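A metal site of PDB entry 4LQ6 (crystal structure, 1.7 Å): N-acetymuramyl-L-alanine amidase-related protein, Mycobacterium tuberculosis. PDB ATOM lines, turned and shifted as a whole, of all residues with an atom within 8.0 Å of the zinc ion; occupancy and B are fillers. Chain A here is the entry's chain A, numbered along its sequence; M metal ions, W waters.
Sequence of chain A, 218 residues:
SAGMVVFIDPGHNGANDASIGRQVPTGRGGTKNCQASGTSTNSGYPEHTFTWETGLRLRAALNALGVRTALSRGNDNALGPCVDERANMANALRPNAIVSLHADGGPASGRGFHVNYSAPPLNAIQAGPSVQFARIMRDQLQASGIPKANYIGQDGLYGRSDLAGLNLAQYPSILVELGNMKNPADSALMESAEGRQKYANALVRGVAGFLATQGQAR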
ATOM      1  N   PRO A  10      -2.483  10.067 -20.119  1.00  0.00           N
ATOM      2  CA  PRO A  10      -1.376  10.967 -20.489  1.00  0.00           C
ATOM      3  C   PRO A  10      -1.701  11.570 -21.856  1.00  0.00           C
ATOM      4  O   PRO A  10      -1.774  10.872 -22.874  1.00  0.00           O
ATOM      5  CB  PRO A  10      -0.149  10.053 -20.579  1.00  0.00           C
ATOM      6  CG  PRO A  10      -0.619   8.679 -20.272  1.00  0.00           C
ATOM      7  CD  PRO A  10      -2.099   8.632 -20.226  1.00  0.00           C
ATOM      8  N   GLY A  11      -1.962  12.879 -21.850  1.00  0.00           N
ATOM      9  CA  GLY A  11      -2.419  13.575 -23.046  1.00  0.00           C
ATOM     10  C   GLY A  11      -1.531  13.392 -24.258  1.00  0.00           C
ATOM     11  O   GLY A  11      -0.294  13.286 -24.127  1.00  0.00           O
ATOM     12  N   HIS A  12      -2.164  13.395 -25.430  1.00  0.00           N
ATOM     13  CA  HIS A  12      -1.470  13.334 -26.718  1.00  0.00           C
ATOM     14  C   HIS A  12      -0.882  11.969 -27.026  1.00  0.00           C
ATOM     15  O   HIS A  12      -1.052  11.026 -26.240  1.00  0.00           O
ATOM     16  CB  HIS A  12      -0.453  14.498 -26.871  1.00  0.00           C
ATOM     17  CG  HIS A  12      -1.073  15.820 -26.584  1.00  0.00           C
ATOM     18  ND1 HIS A  12      -1.801  16.507 -27.555  1.00  0.00           N
ATOM     19  CD2 HIS A  12      -1.155  16.482 -25.404  1.00  0.00           C
ATOM     20  CE1 HIS A  12      -2.272  17.595 -26.946  1.00  0.00           C
ATOM     21  NE2 HIS A  12      -1.896  17.629 -25.654  1.00  0.00           N
ATOM     22  N   GLN A  35      -7.037  14.389 -32.652  1.00  0.00           N
ATOM     23  CA  GLN A  35      -5.957  14.669 -31.702  1.00  0.00           C
ATOM     24  C   GLN A  35      -5.243  15.946 -32.109  1.00  0.00           C
ATOM     25  O   GLN A  35      -5.407  16.442 -33.215  1.00  0.00           O
ATOM     26  CB  GLN A  35      -4.899  13.536 -31.717  1.00  0.00           C
ATOM     27  CG  GLN A  35      -5.005  12.498 -30.604  1.00  0.00           C
ATOM     28  CD  GLN A  35      -4.923  13.087 -29.224  1.00  0.00           C
ATOM     29  OE1 GLN A  35      -4.474  14.234 -29.012  1.00  0.00           O
ATOM     30  NE2 GLN A  35      -5.398  12.328 -28.262  1.00  0.00           N
ATOM     31  N   ALA A  36      -4.404  16.436 -31.212  1.00  0.00           N
ATOM     32  CA  ALA A  36      -3.533  17.589 -31.410  1.00  0.00           C
ATOM     33  C   ALA A  36      -2.166  17.127 -31.038  1.00  0.00           C
ATOM     34  O   ALA A  36      -2.041  16.221 -30.211  1.00  0.00           O
ATOM     35  CB  ALA A  36      -3.965  18.742 -30.527  1.00  0.00           C
ATOM     36  N   SER A  37      -1.109  17.688 -31.685  1.00  0.00           N
ATOM     37  CA  SER A  37       0.262  17.242 -31.399  1.00  0.00           C
ATOM     38  C   SER A  37       0.671  17.536 -29.986  1.00  0.00           C
ATOM     39  O   SER A  37       1.425  16.779 -29.376  1.00  0.00           O
ATOM     40  CB  SER A  37       1.245  17.910 -32.355  1.00  0.00           C
ATOM     41  OG  SER A  37       1.111  19.324 -32.300  1.00  0.00           O
ATOM     42  N   GLY A  38       0.194  18.662 -29.458  1.00  0.00           N
ATOM     43  CA  GLY A  38       0.654  19.046 -28.137  1.00  0.00           C
ATOM     44  C   GLY A  38       1.819  20.023 -28.308  1.00  0.00           C
ATOM     45  O   GLY A  38       2.292  20.252 -29.414  1.00  0.00           O
ATOM     46  N   THR A  39       2.281  20.573 -27.193  1.00  0.00           N
ATOM     47  CA  THR A  39       3.331  21.598 -27.178  1.00  0.00           C
ATOM     48  C   THR A  39       4.666  21.026 -26.762  1.00  0.00           C
ATOM     49  O   THR A  39       4.873  19.810 -26.787  1.00  0.00           O
ATOM     50  CB  THR A  39       2.838  22.809 -26.381  1.00  0.00           C
ATOM     51  OG1 THR A  39       3.765  23.897 -26.522  1.00  0.00           O
ATOM     52  CG2 THR A  39       2.613  22.499 -24.902  1.00  0.00           C
ATOM     53  N   GLU A  47       5.365  17.793 -24.856  1.00  0.00           N
ATOM     54  CA  GLU A  47       4.248  17.579 -23.937  1.00  0.00           C
ATOM     55  C   GLU A  47       3.907  16.085 -23.840  1.00  0.00           C
ATOM     56  O   GLU A  47       3.689  15.566 -22.740  1.00  0.00           O
ATOM     57  CB  GLU A  47       3.011  18.362 -24.418  1.00  0.00           C
ATOM     58  CG  GLU A  47       1.799  18.173 -23.484  1.00  0.00           C
ATOM     59  CD  GLU A  47       0.558  18.886 -23.964  1.00  0.00           C
ATOM     60  OE1 GLU A  47       0.648  19.605 -24.983  1.00  0.00           O
ATOM     61  OE2 GLU A  47      -0.512  18.704 -23.335  1.00  0.00           O
ATOM     62  N   HIS A  48       3.860  15.391 -24.976  1.00  0.00           N
ATOM     63  CA  HIS A  48       3.477  13.980 -24.951  1.00  0.00           C
ATOM     64  C   HIS A  48       4.397  13.133 -24.065  1.00  0.00           C
ATOM     65  O   HIS A  48       3.942  12.154 -23.486  1.00  0.00           O
ATOM     66  CB  HIS A  48       3.347  13.402 -26.366  1.00  0.00           C
ATOM     67  CG  HIS A  48       4.632  13.198 -27.113  1.00  0.00           C
ATOM     68  ND1 HIS A  48       5.407  12.060 -26.937  1.00  0.00           N
ATOM     69  CD2 HIS A  48       5.197  13.971 -28.072  1.00  0.00           C
ATOM     70  CE1 HIS A  48       6.437  12.192 -27.766  1.00  0.00           C
ATOM     71  NE2 HIS A  48       6.358  13.335 -28.462  1.00  0.00           N
ATOM     72  N   THR A  51       3.696  14.194 -20.234  1.00  0.00           N
ATOM     73  CA  THR A  51       2.457  13.589 -19.680  1.00  0.00           C
ATOM     74  C   THR A  51       2.616  12.092 -19.488  1.00  0.00           C
ATOM     75  O   THR A  51       2.113  11.541 -18.509  1.00  0.00           O
ATOM     76  CB  THR A  51       1.271  13.906 -20.593  1.00  0.00           C
ATOM     77  OG1 THR A  51       1.466  13.270 -21.866  1.00  0.00           O
ATOM     78  CG2 THR A  51       1.092  15.418 -20.788  1.00  0.00           C
ATOM     79  N   SER A 100      -6.961  13.228 -16.785  1.00  0.00           N
ATOM     80  CA  SER A 100      -6.194  13.465 -18.011  1.00  0.00           C
ATOM     81  C   SER A 100      -5.069  14.463 -17.678  1.00  0.00           C
ATOM     82  O   SER A 100      -5.307  15.397 -16.902  1.00  0.00           O
ATOM     83  CB  SER A 100      -7.104  14.000 -19.107  1.00  0.00           C
ATOM     84  OG  SER A 100      -6.346  14.295 -20.269  1.00  0.00           O
ATOM     85  N   LEU A 101      -3.842  14.167 -18.139  1.00  0.00           N
ATOM     86  CA  LEU A 101      -2.672  14.998 -17.850  1.00  0.00           C
ATOM     87  C   LEU A 101      -2.219  15.720 -19.100  1.00  0.00           C
ATOM     88  O   LEU A 101      -1.998  15.103 -20.131  1.00  0.00           O
ATOM     89  CB  LEU A 101      -1.511  14.125 -17.346  1.00  0.00           C
ATOM     90  CG  LEU A 101      -1.813  13.246 -16.125  1.00  0.00           C
ATOM     91  CD1 LEU A 101      -0.513  12.603 -15.618  1.00  0.00           C
ATOM     92  CD2 LEU A 101      -2.483  14.081 -15.039  1.00  0.00           C
ATOM     93  N   HIS A 102      -2.027  17.043 -18.999  1.00  0.00           N
ATOM     94  CA  HIS A 102      -1.603  17.862 -20.113  1.00  0.00           C
ATOM     95  C   HIS A 102      -0.645  18.949 -19.598  1.00  0.00           C
ATOM     96  O   HIS A 102      -0.466  19.106 -18.396  1.00  0.00           O
ATOM     97  CB  HIS A 102      -2.846  18.525 -20.742  1.00  0.00           C
ATOM     98  CG  HIS A 102      -3.588  17.636 -21.706  1.00  0.00           C
ATOM     99  ND1 HIS A 102      -3.434  17.768 -23.078  1.00  0.00           N
ATOM    100  CD2 HIS A 102      -4.466  16.643 -21.448  1.00  0.00           C
ATOM    101  CE1 HIS A 102      -4.202  16.833 -23.612  1.00  0.00           C
ATOM    102  NE2 HIS A 102      -4.831  16.112 -22.653  1.00  0.00           N
ATOM    103  N   ALA A 103       0.025  19.659 -20.514  1.00  0.00           N
ATOM    104  CA  ALA A 103       0.831  20.858 -20.203  1.00  0.00           C
ATOM    105  C   ALA A 103       0.477  21.873 -21.267  1.00  0.00           C
ATOM    106  O   ALA A 103       0.126  21.517 -22.386  1.00  0.00           O
ATOM    107  CB  ALA A 103       2.311  20.548 -20.241  1.00  0.00           C
ATOM    108  N   ASP A 104       0.512  23.133 -20.892  1.00  0.00           N
ATOM    109  CA  ASP A 104       0.043  24.176 -21.794  1.00  0.00           C
ATOM    110  C   ASP A 104       1.147  24.860 -22.551  1.00  0.00           C
ATOM    111  O   ASP A 104       2.322  24.768 -22.181  1.00  0.00           O
ATOM    112  CB  ASP A 104      -0.696  25.213 -20.944  1.00  0.00           C
ATOM    113  CG  ASP A 104      -1.774  26.014 -21.632  1.00  0.00           C
ATOM    114  OD1 ASP A 104      -2.083  25.705 -22.809  1.00  0.00           O
ATOM    115  OD2 ASP A 104      -2.265  26.973 -21.018  1.00  0.00           O
ATOM    116  N   GLY A 105       0.741  25.557 -23.610  1.00  0.00           N
ATOM    117  CA  GLY A 105       1.654  26.378 -24.391  1.00  0.00           C
ATOM    118  C   GLY A 105       1.139  27.798 -24.317  1.00  0.00           C
ATOM    119  O   GLY A 105       0.269  28.181 -25.090  1.00  0.00           O
ATOM    120  N   LEU A 175      -9.370  17.286 -16.317  1.00  0.00           N
ATOM    121  CA  LEU A 175      -8.213  17.369 -17.212  1.00  0.00           C
ATOM    122  C   LEU A 175      -7.304  18.416 -16.593  1.00  0.00           C
ATOM    123  O   LEU A 175      -7.678  19.601 -16.440  1.00  0.00           O
ATOM    124  CB  LEU A 175      -8.648  17.703 -18.667  1.00  0.00           C
ATOM    125  CG  LEU A 175      -7.487  17.732 -19.668  1.00  0.00           C
ATOM    126  CD1 LEU A 175      -7.998  17.424 -21.067  1.00  0.00           C
ATOM    127  CD2 LEU A 175      -6.745  19.105 -19.626  1.00  0.00           C
ATOM    128  N   VAL A 176      -6.100  17.968 -16.168  1.00  0.00           N
ATOM    129  CA  VAL A 176      -5.203  18.836 -15.436  1.00  0.00           C
ATOM    130  C   VAL A 176      -4.126  19.373 -16.354  1.00  0.00           C
ATOM    131  O   VAL A 176      -3.366  18.598 -16.931  1.00  0.00           O
ATOM    132  CB  VAL A 176      -4.576  18.088 -14.212  1.00  0.00           C
ATOM    133  CG1 VAL A 176      -3.670  19.031 -13.417  1.00  0.00           C
ATOM    134  CG2 VAL A 176      -5.653  17.500 -13.292  1.00  0.00           C
ATOM    135  N   GLU A 177      -4.068  20.708 -16.513  1.00  0.00           N
ATOM    136  CA  GLU A 177      -2.953  21.355 -17.210  1.00  0.00           C
ATOM    137  C   GLU A 177      -1.944  21.667 -16.103  1.00  0.00           C
ATOM    138  O   GLU A 177      -2.181  22.544 -15.260  1.00  0.00           O
ATOM    139  CB  GLU A 177      -3.409  22.636 -17.904  1.00  0.00           C
ATOM    140  CG  GLU A 177      -4.259  22.334 -19.119  1.00  0.00           C
ATOM    141  CD  GLU A 177      -3.486  21.897 -20.339  1.00  0.00           C
ATOM    142  OE1 GLU A 177      -2.234  21.865 -20.276  1.00  0.00           O
ATOM    143  OE2 GLU A 177      -4.122  21.637 -21.387  1.00  0.00           O
ATOM    144  N   MET A 181       4.517  24.892 -20.527  1.00  0.00           N
ATOM    145  CA  MET A 181       5.846  24.447 -21.016  1.00  0.00           C
ATOM    146  C   MET A 181       6.776  25.547 -21.479  1.00  0.00           C
ATOM    147  O   MET A 181       7.985  25.327 -21.535  1.00  0.00           O
ATOM    148  CB  MET A 181       5.736  23.407 -22.142  1.00  0.00           C
ATOM    149  CG  MET A 181       4.774  22.270 -21.800  1.00  0.00           C
ATOM    150  SD  MET A 181       5.106  20.763 -22.760  1.00  0.00           S
ATOM    151  CE  MET A 181       6.302  19.929 -21.747  1.00  0.00           C
HETATM  152 ZN    ZN M   1      -2.366  19.038 -24.268  1.00  0.00          ZN
HETATM  153 PT    PT M   2      -9.205  17.974 -26.045  1.00  0.00          PT
HETATM  154  O   HOH W   1      -1.549  20.602 -25.796  1.00  0.00           O
HETATM  155  O   HOH W   2      -2.537  20.889 -23.247  1.00  0.00           O
HETATM  156  O   HOH W   3      -4.159  19.654 -25.297  1.00  0.00           O
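The backbone NH (N) of His 102 lies within hydrogen-bond range of the backbone carbonyl oxygen (O) of Val 176, 2.9 Å away. A ring nitrogen (ND1) of His 12 is in hydrogen-bond range of the backbone NH (N) of Gly 38, 3.5 Å away. The side-chain carboxylate of Glu 47 sits close to the backbone NH of Ala 103 (3.0 Å). The backbone carbonyl oxygen of Thr 39 lies within hydrogen-bond range of the backbone NH of Glu 47, at 2.8 Å. The side-chain hydroxyl of Thr 51 sits close to the backbone carbonyl oxygen of Glu 47 (3.3 Å). ND1 of His 12 lies within hydrogen-bond range of O of Ala 36, at 2.7 Å. The side-chain carboxylate (OE1) of Glu 177 lies close to the backbone NH (N) of Ala 103 (3.2 Å). A ring nitrogen (NE2) of His 102 sits close to the side-chain hydroxyl (OG) of Ser 100 (3.4 Å).
Ala 103 touches the zinc ion. Within 4 Å of the zinc ion: His 12, Glu 47, His 102 and Ala 103. The nearest printed residue that does not touch the zinc ion is Glu 177 (4.3 Å).
The zinc ion is bound by NE2 of His 12 (2.0 Å). ND1 of His 102 is bound to the zinc ion (2.0 Å). The zinc ion is bound by OE2 of Glu 47 (2.1 Å). Water W2 binds the zinc ion (2.1 Å). The zinc ion is bound by water W3 (2.2 Å). Water W1 is bound to the zinc ion (2.3 Å). The zinc ion has six donor atoms within binding distance.
Water W2 lies within hydrogen-bond range of the side-chain carboxylate (OE2) of Glu 177 (2.6 Å) and the backbone carbonyl oxygen (O) of Ala 103 (2.9 Å).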
